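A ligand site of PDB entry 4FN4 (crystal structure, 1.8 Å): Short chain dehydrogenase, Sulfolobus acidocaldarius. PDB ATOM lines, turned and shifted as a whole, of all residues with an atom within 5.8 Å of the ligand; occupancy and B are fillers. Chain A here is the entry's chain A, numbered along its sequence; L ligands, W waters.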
ATOM      1  N   THR A  13      -7.151 -12.096  -1.968  1.00  0.00           N
ATOM      2  CA  THR A  13      -6.321 -10.891  -1.944  1.00  0.00           C
ATOM      3  C   THR A  13      -6.866  -9.916  -0.896  1.00  0.00           C
ATOM      4  O   THR A  13      -8.047  -9.963  -0.538  1.00  0.00           O
ATOM      5  CB  THR A  13      -6.266 -10.219  -3.339  1.00  0.00           C
ATOM      6  OG1 THR A  13      -7.552  -9.715  -3.712  1.00  0.00           O
ATOM      7  CG2 THR A  13      -5.806 -11.262  -4.378  1.00  0.00           C
ATOM      8  N   GLY A  14      -5.983  -9.055  -0.384  1.00  0.00           N
ATOM      9  CA  GLY A  14      -6.366  -8.137   0.665  1.00  0.00           C
ATOM     10  C   GLY A  14      -6.699  -8.930   1.925  1.00  0.00           C
ATOM     11  O   GLY A  14      -7.543  -8.522   2.728  1.00  0.00           O
ATOM     12  N   ALA A  15      -6.030 -10.070   2.113  1.00  0.00           N
ATOM     13  CA  ALA A  15      -6.318 -10.952   3.234  1.00  0.00           C
ATOM     14  C   ALA A  15      -5.948 -10.452   4.632  1.00  0.00           C
ATOM     15  O   ALA A  15      -6.396 -11.034   5.617  1.00  0.00           O
ATOM     16  CB  ALA A  15      -5.677 -12.322   3.003  1.00  0.00           C
ATOM     17  N   GLY A  16      -5.165  -9.393   4.728  1.00  0.00           N
ATOM     18  CA  GLY A  16      -4.755  -8.903   6.027  1.00  0.00           C
ATOM     19  C   GLY A  16      -5.729  -8.086   6.858  1.00  0.00           C
ATOM     20  O   GLY A  16      -5.458  -7.804   8.037  1.00  0.00           O
ATOM     21  N   SER A  17      -6.870  -7.709   6.287  1.00  0.00           N
ATOM     22  CA  SER A  17      -7.819  -6.888   7.039  1.00  0.00           C
ATOM     23  C   SER A  17      -9.241  -6.996   6.514  1.00  0.00           C
ATOM     24  O   SER A  17      -9.481  -7.518   5.431  1.00  0.00           O
ATOM     25  CB  SER A  17      -7.361  -5.417   6.975  1.00  0.00           C
ATOM     26  OG  SER A  17      -8.316  -4.527   7.533  1.00  0.00           O
ATOM     27  N   GLY A  18     -10.176  -6.489   7.314  1.00  0.00           N
ATOM     28  CA  GLY A  18     -11.580  -6.450   6.957  1.00  0.00           C
ATOM     29  C   GLY A  18     -12.191  -7.680   6.326  1.00  0.00           C
ATOM     30  O   GLY A  18     -12.081  -8.776   6.857  1.00  0.00           O
ATOM     31  N   ILE A  19     -12.868  -7.469   5.202  1.00  0.00           N
ATOM     32  CA  ILE A  19     -13.549  -8.544   4.484  1.00  0.00           C
ATOM     33  C   ILE A  19     -12.575  -9.652   4.074  1.00  0.00           C
ATOM     34  O   ILE A  19     -12.872 -10.834   4.237  1.00  0.00           O
ATOM     35  CB  ILE A  19     -14.273  -7.959   3.238  1.00  0.00           C
ATOM     36  CG1 ILE A  19     -15.351  -6.982   3.710  1.00  0.00           C
ATOM     37  CG2 ILE A  19     -14.879  -9.084   2.397  1.00  0.00           C
ATOM     38  CD1 ILE A  19     -16.030  -6.186   2.589  1.00  0.00           C
ATOM     39  N   GLY A  20     -11.406  -9.269   3.561  1.00  0.00           N
ATOM     40  CA  GLY A  20     -10.425 -10.249   3.145  1.00  0.00           C
ATOM     41  C   GLY A  20     -10.002 -11.174   4.272  1.00  0.00           C
ATOM     42  O   GLY A  20      -9.889 -12.389   4.086  1.00  0.00           O
ATOM     43  N   VAL A  37      -3.029 -13.261   0.166  1.00  0.00           N
ATOM     44  CA  VAL A  37      -2.242 -12.230  -0.526  1.00  0.00           C
ATOM     45  C   VAL A  37      -2.523 -10.879   0.141  1.00  0.00           C
ATOM     46  O   VAL A  37      -3.674 -10.466   0.267  1.00  0.00           O
ATOM     47  CB  VAL A  37      -2.603 -12.153  -2.023  1.00  0.00           C
ATOM     48  CG1 VAL A  37      -1.800 -11.035  -2.704  1.00  0.00           C
ATOM     49  CG2 VAL A  37      -2.295 -13.484  -2.706  1.00  0.00           C
ATOM     50  N   GLU A  38      -1.457 -10.197   0.561  1.00  0.00           N
ATOM     51  CA  GLU A  38      -1.603  -8.924   1.256  1.00  0.00           C
ATOM     52  C   GLU A  38      -0.390  -8.041   1.019  1.00  0.00           C
ATOM     53  O   GLU A  38       0.746  -8.526   0.945  1.00  0.00           O
ATOM     54  CB  GLU A  38      -1.810  -9.200   2.747  1.00  0.00           C
ATOM     55  CG  GLU A  38      -1.691  -8.009   3.696  1.00  0.00           C
ATOM     56  CD  GLU A  38      -2.721  -6.938   3.445  1.00  0.00           C
ATOM     57  OE1 GLU A  38      -3.926  -7.277   3.277  1.00  0.00           O
ATOM     58  OE2 GLU A  38      -2.334  -5.745   3.438  1.00  0.00           O
ATOM     59  N   LEU A  39      -0.631  -6.741   0.907  1.00  0.00           N
ATOM     60  CA  LEU A  39       0.416  -5.750   0.675  1.00  0.00           C
ATOM     61  C   LEU A  39       1.276  -5.467   1.910  1.00  0.00           C
ATOM     62  O   LEU A  39       2.498  -5.339   1.815  1.00  0.00           O
ATOM     63  CB  LEU A  39      -0.223  -4.430   0.216  1.00  0.00           C
ATOM     64  CG  LEU A  39       0.669  -3.220  -0.049  1.00  0.00           C
ATOM     65  CD1 LEU A  39       1.397  -3.382  -1.374  1.00  0.00           C
ATOM     66  CD2 LEU A  39      -0.194  -1.953  -0.090  1.00  0.00           C
ATOM     67  N   LEU A  40       0.621  -5.373   3.070  1.00  0.00           N
ATOM     68  CA  LEU A  40       1.315  -5.057   4.321  1.00  0.00           C
ATOM     69  C   LEU A  40       1.801  -6.283   5.076  1.00  0.00           C
ATOM     70  O   LEU A  40       1.020  -7.174   5.420  1.00  0.00           O
ATOM     71  CB  LEU A  40       0.403  -4.216   5.208  1.00  0.00           C
ATOM     72  CG  LEU A  40      -0.080  -2.915   4.553  1.00  0.00           C
ATOM     73  CD1 LEU A  40      -1.027  -2.183   5.487  1.00  0.00           C
ATOM     74  CD2 LEU A  40       1.112  -2.037   4.194  1.00  0.00           C
ATOM     75  N   ARG A  43       0.279  -7.211   8.697  1.00  0.00           N
ATOM     76  CA  ARG A  43      -1.082  -7.734   8.543  1.00  0.00           C
ATOM     77  C   ARG A  43      -1.031  -9.139   7.951  1.00  0.00           C
ATOM     78  O   ARG A  43      -1.781 -10.007   8.369  1.00  0.00           O
ATOM     79  CB  ARG A  43      -1.914  -6.826   7.639  1.00  0.00           C
ATOM     80  CG  ARG A  43      -2.212  -5.474   8.244  1.00  0.00           C
ATOM     81  CD  ARG A  43      -3.156  -4.684   7.353  1.00  0.00           C
ATOM     82  NE  ARG A  43      -3.580  -3.446   7.991  1.00  0.00           N
ATOM     83  CZ  ARG A  43      -4.427  -2.576   7.445  1.00  0.00           C
ATOM     84  NH1 ARG A  43      -4.946  -2.825   6.248  1.00  0.00           N
ATOM     85  NH2 ARG A  43      -4.771  -1.472   8.092  1.00  0.00           N
ATOM     86  N   ALA A  63       2.335  -9.128  -1.569  1.00  0.00           N
ATOM     87  CA  ALA A  63       2.335  -8.601  -2.922  1.00  0.00           C
ATOM     88  C   ALA A  63       1.428  -7.396  -3.113  1.00  0.00           C
ATOM     89  O   ALA A  63       0.524  -7.142  -2.308  1.00  0.00           O
ATOM     90  CB  ALA A  63       1.905  -9.725  -3.886  1.00  0.00           C
ATOM     91  N   ASP A  64       1.698  -6.650  -4.179  1.00  0.00           N
ATOM     92  CA  ASP A  64       0.914  -5.464  -4.547  1.00  0.00           C
ATOM     93  C   ASP A  64       0.100  -5.914  -5.758  1.00  0.00           C
ATOM     94  O   ASP A  64       0.649  -6.056  -6.857  1.00  0.00           O
ATOM     95  CB  ASP A  64       1.855  -4.322  -4.939  1.00  0.00           C
ATOM     96  CG  ASP A  64       1.112  -3.034  -5.265  1.00  0.00           C
ATOM     97  OD1 ASP A  64      -0.083  -3.100  -5.635  1.00  0.00           O
ATOM     98  OD2 ASP A  64       1.731  -1.953  -5.142  1.00  0.00           O
ATOM     99  N   VAL A  65      -1.193  -6.146  -5.566  1.00  0.00           N
ATOM    100  CA  VAL A  65      -2.026  -6.632  -6.670  1.00  0.00           C
ATOM    101  C   VAL A  65      -2.148  -5.686  -7.862  1.00  0.00           C
ATOM    102  O   VAL A  65      -2.641  -6.097  -8.924  1.00  0.00           O
ATOM    103  CB  VAL A  65      -3.448  -7.035  -6.180  1.00  0.00           C
ATOM    104  CG1 VAL A  65      -3.321  -8.088  -5.059  1.00  0.00           C
ATOM    105  CG2 VAL A  65      -4.210  -5.819  -5.689  1.00  0.00           C
ATOM    106  N   SER A  66      -1.705  -4.438  -7.719  1.00  0.00           N
ATOM    107  CA  SER A  66      -1.786  -3.508  -8.841  1.00  0.00           C
ATOM    108  C   SER A  66      -0.595  -3.705  -9.788  1.00  0.00           C
ATOM    109  O   SER A  66      -0.527  -3.093 -10.847  1.00  0.00           O
ATOM    110  CB  SER A  66      -1.813  -2.055  -8.344  1.00  0.00           C
ATOM    111  OG  SER A  66      -0.546  -1.657  -7.835  1.00  0.00           O
ATOM    112  N   ASN A  90     -10.900 -11.909  -5.771  1.00  0.00           N
ATOM    113  CA  ASN A  90     -10.296 -10.607  -6.038  1.00  0.00           C
ATOM    114  C   ASN A  90     -10.987  -9.645  -5.078  1.00  0.00           C
ATOM    115  O   ASN A  90     -12.000  -9.056  -5.390  1.00  0.00           O
ATOM    116  CB  ASN A  90     -10.538 -10.194  -7.494  1.00  0.00           C
ATOM    117  CG  ASN A  90      -9.665 -10.987  -8.448  1.00  0.00           C
ATOM    118  OD1 ASN A  90      -8.474 -11.131  -8.202  1.00  0.00           O
ATOM    119  ND2 ASN A  90     -10.251 -11.509  -9.515  1.00  0.00           N
ATOM    120  N   ASN A  91     -10.379  -9.483  -3.908  1.00  0.00           N
ATOM    121  CA  ASN A  91     -10.970  -8.679  -2.850  1.00  0.00           C
ATOM    122  C   ASN A  91     -10.275  -7.393  -2.441  1.00  0.00           C
ATOM    123  O   ASN A  91     -10.930  -6.467  -1.986  1.00  0.00           O
ATOM    124  CB  ASN A  91     -11.158  -9.603  -1.638  1.00  0.00           C
ATOM    125  CG  ASN A  91     -11.539  -8.849  -0.396  1.00  0.00           C
ATOM    126  OD1 ASN A  91     -10.681  -8.529   0.440  1.00  0.00           O
ATOM    127  ND2 ASN A  91     -12.817  -8.536  -0.275  1.00  0.00           N
ATOM    128  N   ALA A  92      -8.956  -7.335  -2.590  1.00  0.00           N
ATOM    129  CA  ALA A  92      -8.212  -6.135  -2.228  1.00  0.00           C
ATOM    130  C   ALA A  92      -8.746  -4.896  -2.933  1.00  0.00           C
ATOM    131  O   ALA A  92      -9.124  -4.918  -4.089  1.00  0.00           O
ATOM    132  CB  ALA A  92      -6.745  -6.317  -2.588  1.00  0.00           C
ATOM    133  N   GLY A  93      -8.767  -3.778  -2.200  1.00  0.00           N
ATOM    134  CA  GLY A  93      -9.246  -2.544  -2.792  1.00  0.00           C
ATOM    135  C   GLY A  93      -8.966  -1.399  -1.852  1.00  0.00           C
ATOM    136  O   GLY A  93      -8.719  -1.617  -0.667  1.00  0.00           O
ATOM    137  N   ILE A  94      -8.986  -0.182  -2.387  1.00  0.00           N
ATOM    138  CA  ILE A  94      -8.764   1.024  -1.604  1.00  0.00           C
ATOM    139  C   ILE A  94      -9.827   2.054  -1.971  1.00  0.00           C
ATOM    140  O   ILE A  94     -10.429   1.957  -3.044  1.00  0.00           O
ATOM    141  CB  ILE A  94      -7.378   1.649  -1.900  1.00  0.00           C
ATOM    142  CG1 ILE A  94      -7.225   1.900  -3.407  1.00  0.00           C
ATOM    143  CG2 ILE A  94      -6.266   0.706  -1.411  1.00  0.00           C
ATOM    144  CD1 ILE A  94      -5.993   2.718  -3.791  1.00  0.00           C
ATOM    145  N   VAL A 115      -5.436  -0.731  -8.516  1.00  0.00           N
ATOM    146  CA  VAL A 115      -5.695  -1.576  -7.360  1.00  0.00           C
ATOM    147  C   VAL A 115      -7.080  -2.235  -7.368  1.00  0.00           C
ATOM    148  O   VAL A 115      -7.218  -3.425  -7.069  1.00  0.00           O
ATOM    149  CB  VAL A 115      -5.563  -0.772  -6.050  1.00  0.00           C
ATOM    150  CG1 VAL A 115      -5.919  -1.648  -4.870  1.00  0.00           C
ATOM    151  CG2 VAL A 115      -4.144  -0.230  -5.911  1.00  0.00           C
ATOM    152  N   ASN A 116      -8.099  -1.464  -7.741  1.00  0.00           N
ATOM    153  CA  ASN A 116      -9.466  -1.974  -7.713  1.00  0.00           C
ATOM    154  C   ASN A 116      -9.981  -2.700  -8.951  1.00  0.00           C
ATOM    155  O   ASN A 116     -10.949  -3.454  -8.861  1.00  0.00           O
ATOM    156  CB  ASN A 116     -10.428  -0.826  -7.359  1.00  0.00           C
ATOM    157  CG  ASN A 116     -10.206  -0.287  -5.953  1.00  0.00           C
ATOM    158  OD1 ASN A 116      -9.229  -0.629  -5.274  1.00  0.00           O
ATOM    159  ND2 ASN A 116     -11.124   0.572  -5.497  1.00  0.00           N
ATOM    160  N   THR A 142     -14.968  -8.811  -5.278  1.00  0.00           N
ATOM    161  CA  THR A 142     -15.613  -7.942  -4.306  1.00  0.00           C
ATOM    162  C   THR A 142     -15.765  -6.566  -4.940  1.00  0.00           C
ATOM    163  O   THR A 142     -14.780  -5.823  -5.070  1.00  0.00           O
ATOM    164  CB  THR A 142     -14.795  -7.783  -2.996  1.00  0.00           C
ATOM    165  OG1 THR A 142     -14.505  -9.080  -2.439  1.00  0.00           O
ATOM    166  CG2 THR A 142     -15.610  -6.989  -1.979  1.00  0.00           C
ATOM    167  N   ALA A 143     -16.984  -6.247  -5.360  1.00  0.00           N
ATOM    168  CA  ALA A 143     -17.257  -4.961  -5.969  1.00  0.00           C
ATOM    169  C   ALA A 143     -17.751  -3.995  -4.879  1.00  0.00           C
ATOM    170  O   ALA A 143     -17.090  -3.835  -3.857  1.00  0.00           O
ATOM    171  CB  ALA A 143     -18.313  -5.103  -7.086  1.00  0.00           C
ATOM    172  N   SER A 144     -18.899  -3.361  -5.091  1.00  0.00           N
ATOM    173  CA  SER A 144     -19.442  -2.409  -4.126  1.00  0.00           C
ATOM    174  C   SER A 144     -20.745  -1.900  -4.711  1.00  0.00           C
ATOM    175  O   SER A 144     -20.985  -2.068  -5.897  1.00  0.00           O
ATOM    176  CB  SER A 144     -18.492  -1.209  -3.997  1.00  0.00           C
ATOM    177  OG  SER A 144     -19.127  -0.105  -3.372  1.00  0.00           O
ATOM    178  N   ILE A 145     -21.600  -1.277  -3.895  1.00  0.00           N
ATOM    179  CA  ILE A 145     -22.819  -0.733  -4.482  1.00  0.00           C
ATOM    180  C   ILE A 145     -22.412   0.493  -5.320  1.00  0.00           C
ATOM    181  O   ILE A 145     -23.210   1.031  -6.081  1.00  0.00           O
ATOM    182  CB  ILE A 145     -23.867  -0.338  -3.407  1.00  0.00           C
ATOM    183  CG1 ILE A 145     -23.227   0.489  -2.294  1.00  0.00           C
ATOM    184  CG2 ILE A 145     -24.535  -1.603  -2.846  1.00  0.00           C
ATOM    185  CD1 ILE A 145     -24.259   1.032  -1.303  1.00  0.00           C
ATOM    186  N   TYR A 157     -13.223   5.331  -7.783  1.00  0.00           N
ATOM    187  CA  TYR A 157     -13.768   4.126  -7.150  1.00  0.00           C
ATOM    188  C   TYR A 157     -15.042   3.661  -7.868  1.00  0.00           C
ATOM    189  O   TYR A 157     -15.211   2.478  -8.163  1.00  0.00           O
ATOM    190  CB  TYR A 157     -14.072   4.410  -5.683  1.00  0.00           C
ATOM    191  CG  TYR A 157     -14.384   3.211  -4.828  1.00  0.00           C
ATOM    192  CD1 TYR A 157     -13.367   2.515  -4.155  1.00  0.00           C
ATOM    193  CD2 TYR A 157     -15.710   2.829  -4.593  1.00  0.00           C
ATOM    194  CE1 TYR A 157     -13.671   1.492  -3.251  1.00  0.00           C
ATOM    195  CE2 TYR A 157     -16.014   1.806  -3.689  1.00  0.00           C
ATOM    196  CZ  TYR A 157     -14.998   1.152  -3.022  1.00  0.00           C
ATOM    197  OH  TYR A 157     -15.326   0.201  -2.071  1.00  0.00           O
ATOM    198  N   LYS A 161     -15.279   0.120  -9.788  1.00  0.00           N
ATOM    199  CA  LYS A 161     -16.242  -0.885  -9.363  1.00  0.00           C
ATOM    200  C   LYS A 161     -17.253  -1.225 -10.459  1.00  0.00           C
ATOM    201  O   LYS A 161     -17.678  -2.367 -10.560  1.00  0.00           O
ATOM    202  CB  LYS A 161     -16.941  -0.449  -8.078  1.00  0.00           C
ATOM    203  CG  LYS A 161     -15.996  -0.348  -6.859  1.00  0.00           C
ATOM    204  CD  LYS A 161     -15.358  -1.713  -6.496  1.00  0.00           C
ATOM    205  CE  LYS A 161     -14.631  -1.647  -5.149  1.00  0.00           C
ATOM    206  NZ  LYS A 161     -14.031  -2.963  -4.752  1.00  0.00           N
ATOM    207  N   LEU A 186     -21.531  -7.231  -3.927  1.00  0.00           N
ATOM    208  CA  LEU A 186     -21.565  -5.783  -3.743  1.00  0.00           C
ATOM    209  C   LEU A 186     -21.964  -5.376  -2.317  1.00  0.00           C
ATOM    210  O   LEU A 186     -23.139  -5.292  -1.995  1.00  0.00           O
ATOM    211  CB  LEU A 186     -22.557  -5.165  -4.735  1.00  0.00           C
ATOM    212  CG  LEU A 186     -22.248  -5.130  -6.239  1.00  0.00           C
ATOM    213  CD1 LEU A 186     -21.923  -6.521  -6.787  1.00  0.00           C
ATOM    214  CD2 LEU A 186     -23.456  -4.516  -6.969  1.00  0.00           C
ATOM    215  N   PRO A 187     -20.971  -5.134  -1.454  1.00  0.00           N
ATOM    216  CA  PRO A 187     -21.280  -4.738  -0.075  1.00  0.00           C
ATOM    217  C   PRO A 187     -21.743  -3.274  -0.069  1.00  0.00           C
ATOM    218  O   PRO A 187     -21.472  -2.528  -1.014  1.00  0.00           O
ATOM    219  CB  PRO A 187     -19.945  -4.884   0.650  1.00  0.00           C
ATOM    220  CG  PRO A 187     -19.096  -5.751  -0.263  1.00  0.00           C
ATOM    221  CD  PRO A 187     -19.520  -5.307  -1.632  1.00  0.00           C
ATOM    222  N   GLY A 188     -22.424  -2.885   1.001  1.00  0.00           N
ATOM    223  CA  GLY A 188     -22.881  -1.516   1.149  1.00  0.00           C
ATOM    224  C   GLY A 188     -21.895  -0.786   2.044  1.00  0.00           C
ATOM    225  O   GLY A 188     -20.939  -0.175   1.547  1.00  0.00           O
ATOM    226  N   THR A 189     -22.124  -0.831   3.349  1.00  0.00           N
ATOM    227  CA  THR A 189     -21.239  -0.202   4.319  1.00  0.00           C
ATOM    228  C   THR A 189     -20.813  -1.308   5.276  1.00  0.00           C
ATOM    229  O   THR A 189     -21.654  -1.950   5.896  1.00  0.00           O
ATOM    230  CB  THR A 189     -21.978   0.897   5.111  1.00  0.00           C
ATOM    231  OG1 THR A 189     -23.128   0.340   5.757  1.00  0.00           O
ATOM    232  CG2 THR A 189     -22.425   1.995   4.183  1.00  0.00           C
ATOM    233  N   VAL A 190     -19.508  -1.520   5.389  1.00  0.00           N
ATOM    234  CA  VAL A 190     -18.982  -2.586   6.233  1.00  0.00           C
ATOM    235  C   VAL A 190     -17.898  -2.063   7.180  1.00  0.00           C
ATOM    236  O   VAL A 190     -17.090  -1.225   6.811  1.00  0.00           O
ATOM    237  CB  VAL A 190     -18.354  -3.710   5.353  1.00  0.00           C
ATOM    238  CG1 VAL A 190     -18.033  -4.931   6.202  1.00  0.00           C
ATOM    239  CG2 VAL A 190     -19.316  -4.064   4.218  1.00  0.00           C
ATOM    240  N   LYS A 191     -17.902  -2.578   8.403  1.00  0.00           N
ATOM    241  CA  LYS A 191     -16.911  -2.139   9.388  1.00  0.00           C
ATOM    242  C   LYS A 191     -15.546  -2.744   9.079  1.00  0.00           C
ATOM    243  O   LYS A 191     -15.294  -3.912   9.377  1.00  0.00           O
ATOM    244  CB  LYS A 191     -17.331  -2.565  10.805  1.00  0.00           C
ATOM    245  CG  LYS A 191     -16.419  -1.947  11.876  1.00  0.00           C
ATOM    246  CD  LYS A 191     -16.342  -2.788  13.138  1.00  0.00           C
ATOM    247  CE  LYS A 191     -17.682  -2.942  13.799  1.00  0.00           C
ATOM    248  NZ  LYS A 191     -17.553  -3.775  15.034  1.00  0.00           N
ATOM    249  N   THR A 192     -14.661  -1.935   8.489  1.00  0.00           N
ATOM    250  CA  THR A 192     -13.321  -2.407   8.143  1.00  0.00           C
ATOM    251  C   THR A 192     -12.316  -1.270   8.328  1.00  0.00           C
ATOM    252  O   THR A 192     -12.583  -0.307   9.044  1.00  0.00           O
ATOM    253  CB  THR A 192     -13.246  -2.874   6.676  1.00  0.00           C
ATOM    254  OG1 THR A 192     -13.405  -1.739   5.805  1.00  0.00           O
ATOM    255  CG2 THR A 192     -14.356  -3.906   6.378  1.00  0.00           C
ATOM    256  N   ASN A 193     -11.151  -1.390   7.700  1.00  0.00           N
ATOM    257  CA  ASN A 193     -10.131  -0.356   7.804  1.00  0.00           C
ATOM    258  C   ASN A 193     -10.036   0.503   6.551  1.00  0.00           C
ATOM    259  O   ASN A 193      -9.156   1.347   6.458  1.00  0.00           O
ATOM    260  CB  ASN A 193      -8.743  -0.963   8.039  1.00  0.00           C
ATOM    261  CG  ASN A 193      -8.519  -1.379   9.473  1.00  0.00           C
ATOM    262  OD1 ASN A 193      -8.720  -0.595  10.405  1.00  0.00           O
ATOM    263  ND2 ASN A 193      -8.092  -2.622   9.670  1.00  0.00           N
ATOM    264  N   ILE A 194     -10.937   0.287   5.594  1.00  0.00           N
ATOM    265  CA  ILE A 194     -10.833   1.043   4.341  1.00  0.00           C
ATOM    266  C   ILE A 194     -11.115   2.525   4.508  1.00  0.00           C
ATOM    267  O   ILE A 194     -10.475   3.361   3.870  1.00  0.00           O
ATOM    268  CB  ILE A 194     -11.721   0.427   3.220  1.00  0.00           C
ATOM    269  CG1 ILE A 194     -11.209   0.916   1.865  1.00  0.00           C
ATOM    270  CG2 ILE A 194     -13.199   0.798   3.429  1.00  0.00           C
ATOM    271  CD1 ILE A 194     -11.785   0.182   0.644  1.00  0.00           C
HETATM  272  P1  LIG L   1      -9.596  -3.045   4.377  1.00  0.00           P
HETATM  273  O1  LIG L   1     -10.047  -3.350   5.754  1.00  0.00           O
HETATM  274  O2  LIG L   1      -8.749  -1.829   4.130  1.00  0.00           O
HETATM  275  O3  LIG L   1      -8.880  -4.342   3.835  1.00  0.00           O
HETATM  276  C1  LIG L   1      -8.288  -4.355   2.500  1.00  0.00           C
HETATM  277  C2  LIG L   1      -6.947  -5.016   2.596  1.00  0.00           C
HETATM  278  O4  LIG L   1      -6.435  -4.921   1.209  1.00  0.00           O
HETATM  279  C3  LIG L   1      -5.918  -4.252   3.487  1.00  0.00           C
HETATM  280  O5  LIG L   1      -5.337  -5.178   4.459  1.00  0.00           O
HETATM  281  C4  LIG L   1      -4.903  -3.695   2.533  1.00  0.00           C
HETATM  282  O6  LIG L   1      -3.600  -3.479   2.984  1.00  0.00           O
HETATM  283  C5  LIG L   1      -5.065  -4.632   1.318  1.00  0.00           C
HETATM  284  N1  LIG L   1      -4.637  -3.933   0.133  1.00  0.00           N
HETATM  285  C6  LIG L   1      -4.887  -2.652  -0.354  1.00  0.00           C
HETATM  286  N2  LIG L   1      -4.273  -2.395  -1.488  1.00  0.00           N
HETATM  287  C7  LIG L   1      -3.586  -3.501  -1.820  1.00  0.00           C
HETATM  288  C8  LIG L   1      -2.720  -3.829  -2.946  1.00  0.00           C
HETATM  289  N3  LIG L   1      -2.459  -2.970  -3.909  1.00  0.00           N
HETATM  290  N4  LIG L   1      -2.196  -5.112  -2.920  1.00  0.00           N
HETATM  291  C9  LIG L   1      -2.419  -6.032  -1.961  1.00  0.00           C
HETATM  292  N5  LIG L   1      -3.232  -5.770  -0.860  1.00  0.00           N
HETATM  293  C10 LIG L   1      -3.803  -4.486  -0.827  1.00  0.00           C
HETATM  294  O7  LIG L   1     -10.832  -2.916   3.372  1.00  0.00           O
HETATM  295  P2  LIG L   1     -12.238  -3.756   3.222  1.00  0.00           P
HETATM  296  O8  LIG L   1     -13.279  -2.812   3.611  1.00  0.00           O
HETATM  297  O9  LIG L   1     -12.030  -5.061   3.936  1.00  0.00           O
HETATM  298  O10 LIG L   1     -12.488  -3.945   1.681  1.00  0.00           O
HETATM  299  C11 LIG L   1     -11.827  -4.863   0.825  1.00  0.00           C
HETATM  300  C12 LIG L   1     -12.716  -4.874  -0.381  1.00  0.00           C
HETATM  301  O11 LIG L   1     -14.173  -4.586   0.001  1.00  0.00           O
HETATM  302  C13 LIG L   1     -12.369  -3.724  -1.380  1.00  0.00           C
HETATM  303  O12 LIG L   1     -12.428  -4.190  -2.722  1.00  0.00           O
HETATM  304  C14 LIG L   1     -13.438  -2.652  -1.109  1.00  0.00           C
HETATM  305  O13 LIG L   1     -13.561  -1.740  -2.164  1.00  0.00           O
HETATM  306  C15 LIG L   1     -14.690  -3.547  -0.866  1.00  0.00           C
HETATM  307  N6  LIG L   1     -15.873  -2.825  -0.235  1.00  0.00           N
HETATM  308  C16 LIG L   1     -15.785  -2.352   1.119  1.00  0.00           C
HETATM  309  C17 LIG L   1     -16.807  -1.703   1.699  1.00  0.00           C
HETATM  310  C18 LIG L   1     -16.708  -1.211   3.114  1.00  0.00           C
HETATM  311  O14 LIG L   1     -17.560  -0.380   3.510  1.00  0.00           O
HETATM  312  N7  LIG L   1     -15.734  -1.680   3.911  1.00  0.00           N
HETATM  313  C19 LIG L   1     -18.137  -1.431   0.987  1.00  0.00           C
HETATM  314  C20 LIG L   1     -18.196  -1.952  -0.431  1.00  0.00           C
HETATM  315  C21 LIG L   1     -17.074  -2.626  -0.989  1.00  0.00           C
HETATM  316  O   HOH W   1      -7.714  -0.738   1.805  1.00  0.00           O
HETATM  317  O   HOH W   2     -16.599   1.496   5.373  1.00  0.00           O
HETATM  318  O   HOH W   3     -19.998   0.597  -0.797  1.00  0.00           O
HETATM  319  O   HOH W   4      -6.477  -0.846   5.128  1.00  0.00           O
HETATM  320  O   HOH W   5     -10.206  -6.925   2.887  1.00  0.00           O
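The side-chain hydroxyl (OH) of Tyr 157 is in hydrogen-bond range of an oxygen (O13) of the ligand, at 2.6 Å. An oxygen (O5) of the ligand lies within hydrogen-bond range of the guanidinium group (NH1) of Arg 43, at 3.0 Å. The side-chain hydroxyl of Ser 17 sits at hydrogen-bond distance from an oxygen (O1) of the ligand, at 2.7 Å. N of Val 65 is in hydrogen-bond range of N4 of the ligand, at 3.0 Å. A nitrogen (N7) of the ligand is in hydrogen-bond range of the backbone carbonyl oxygen of Val 190, at 3.2 Å. An oxygen (O1) of the ligand sits at hydrogen-bond distance from the backbone NH of Asn 193 (3.0 Å). The backbone carbonyl oxygen of Asn 91 lies within hydrogen-bond range of an oxygen (O12) of the ligand, at 2.8 Å. An oxygen (O14) of the ligand sits at hydrogen-bond distance from the backbone NH of Val 190, at 2.9 Å. The backbone NH (N) of Ile 19 is in hydrogen-bond range of an oxygen (O9) of the ligand (2.8 Å). An oxygen (O2) of the ligand is in hydrogen-bond range of the backbone NH (N) of Ile 194 (3.4 Å). The side-chain carboxylate (OD1) of Asp 64 sits at hydrogen-bond distance from a nitrogen (N3) of the ligand (2.9 Å). NZ of Lys 161 sits at hydrogen-bond distance from O12 of the ligand (2.9 Å). The backbone NH (N) of Ser 17 sits close to an oxygen (O5) of the ligand (3.5 Å). The backbone NH of Leu 39 sits at hydrogen-bond distance from a nitrogen (N5) of the ligand (3.3 Å). OE2 of Glu 38 lies within hydrogen-bond range of O6 of the ligand (2.6 Å). The side-chain hydroxyl of Thr 192 is in hydrogen-bond range of an oxygen (O8) of the ligand (2.4 Å).
ND2 of Asn 91 sits at hydrogen-bond distance from OG1 of Thr 142, 2.8 Å away. O of Asn 90 is in hydrogen-bond range of N of Thr 142, 3.0 Å away. N of Gly 14 lies within hydrogen-bond range of O of Val 37, 2.8 Å away. N of Ala 63 sits at hydrogen-bond distance from O of Glu 38 (3.0 Å). N of Ile 145 is in hydrogen-bond range of O of Pro 187. The side-chain amide oxygen of Asn 91 sits close to the backbone NH of Gly 20, 3.3 Å away. The backbone NH (N) of Asn 91 is in hydrogen-bond range of the side-chain hydroxyl (OG1) of Thr 13 (2.8 Å). The side-chain amide nitrogen (ND2) of Asn 193 is in hydrogen-bond range of the side-chain hydroxyl (OG) of Ser 17 (2.9 Å).
The backbone carbonyl oxygen of Ala 63 sits close to a nitrogen (N4) of the ligand. Merely in contact with the ligand: Ala 143, Gly 188, Gly 14, Gly 18, Pro 187, Thr 142, Gly 93, Ser 144, Ala 92, Ile 94, Thr 189, Val 115, Gly 16 and Leu 40. Hydrophobic or aromatic side chains within 4 Å of the ligand: Ile 19, Leu 39, Leu 40, Val 65, Ala 92, Ile 94, Val 115, Tyr 157, Pro 187, Val 190 and Ile 194. The nearest printed residue that does not touch the ligand is Ser 66 (4.2 Å).
Water W4 lies within hydrogen-bond range of O2 of the ligand and NH1 of Arg 43. Water W1 bridges an oxygen (O2) of the ligand (2.8 Å) and the backbone carbonyl oxygen of Gly 93 (2.8 Å). Water W2 bridges an oxygen (O14) of the ligand (2.8 Å) and the backbone carbonyl oxygen of Val 190 (3.1 Å). Water W3 lies within hydrogen-bond range of O of Gly 188 (2.6 Å), OG of Ser 144 (2.8 Å) and O of Pro 187 (3.5 Å).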
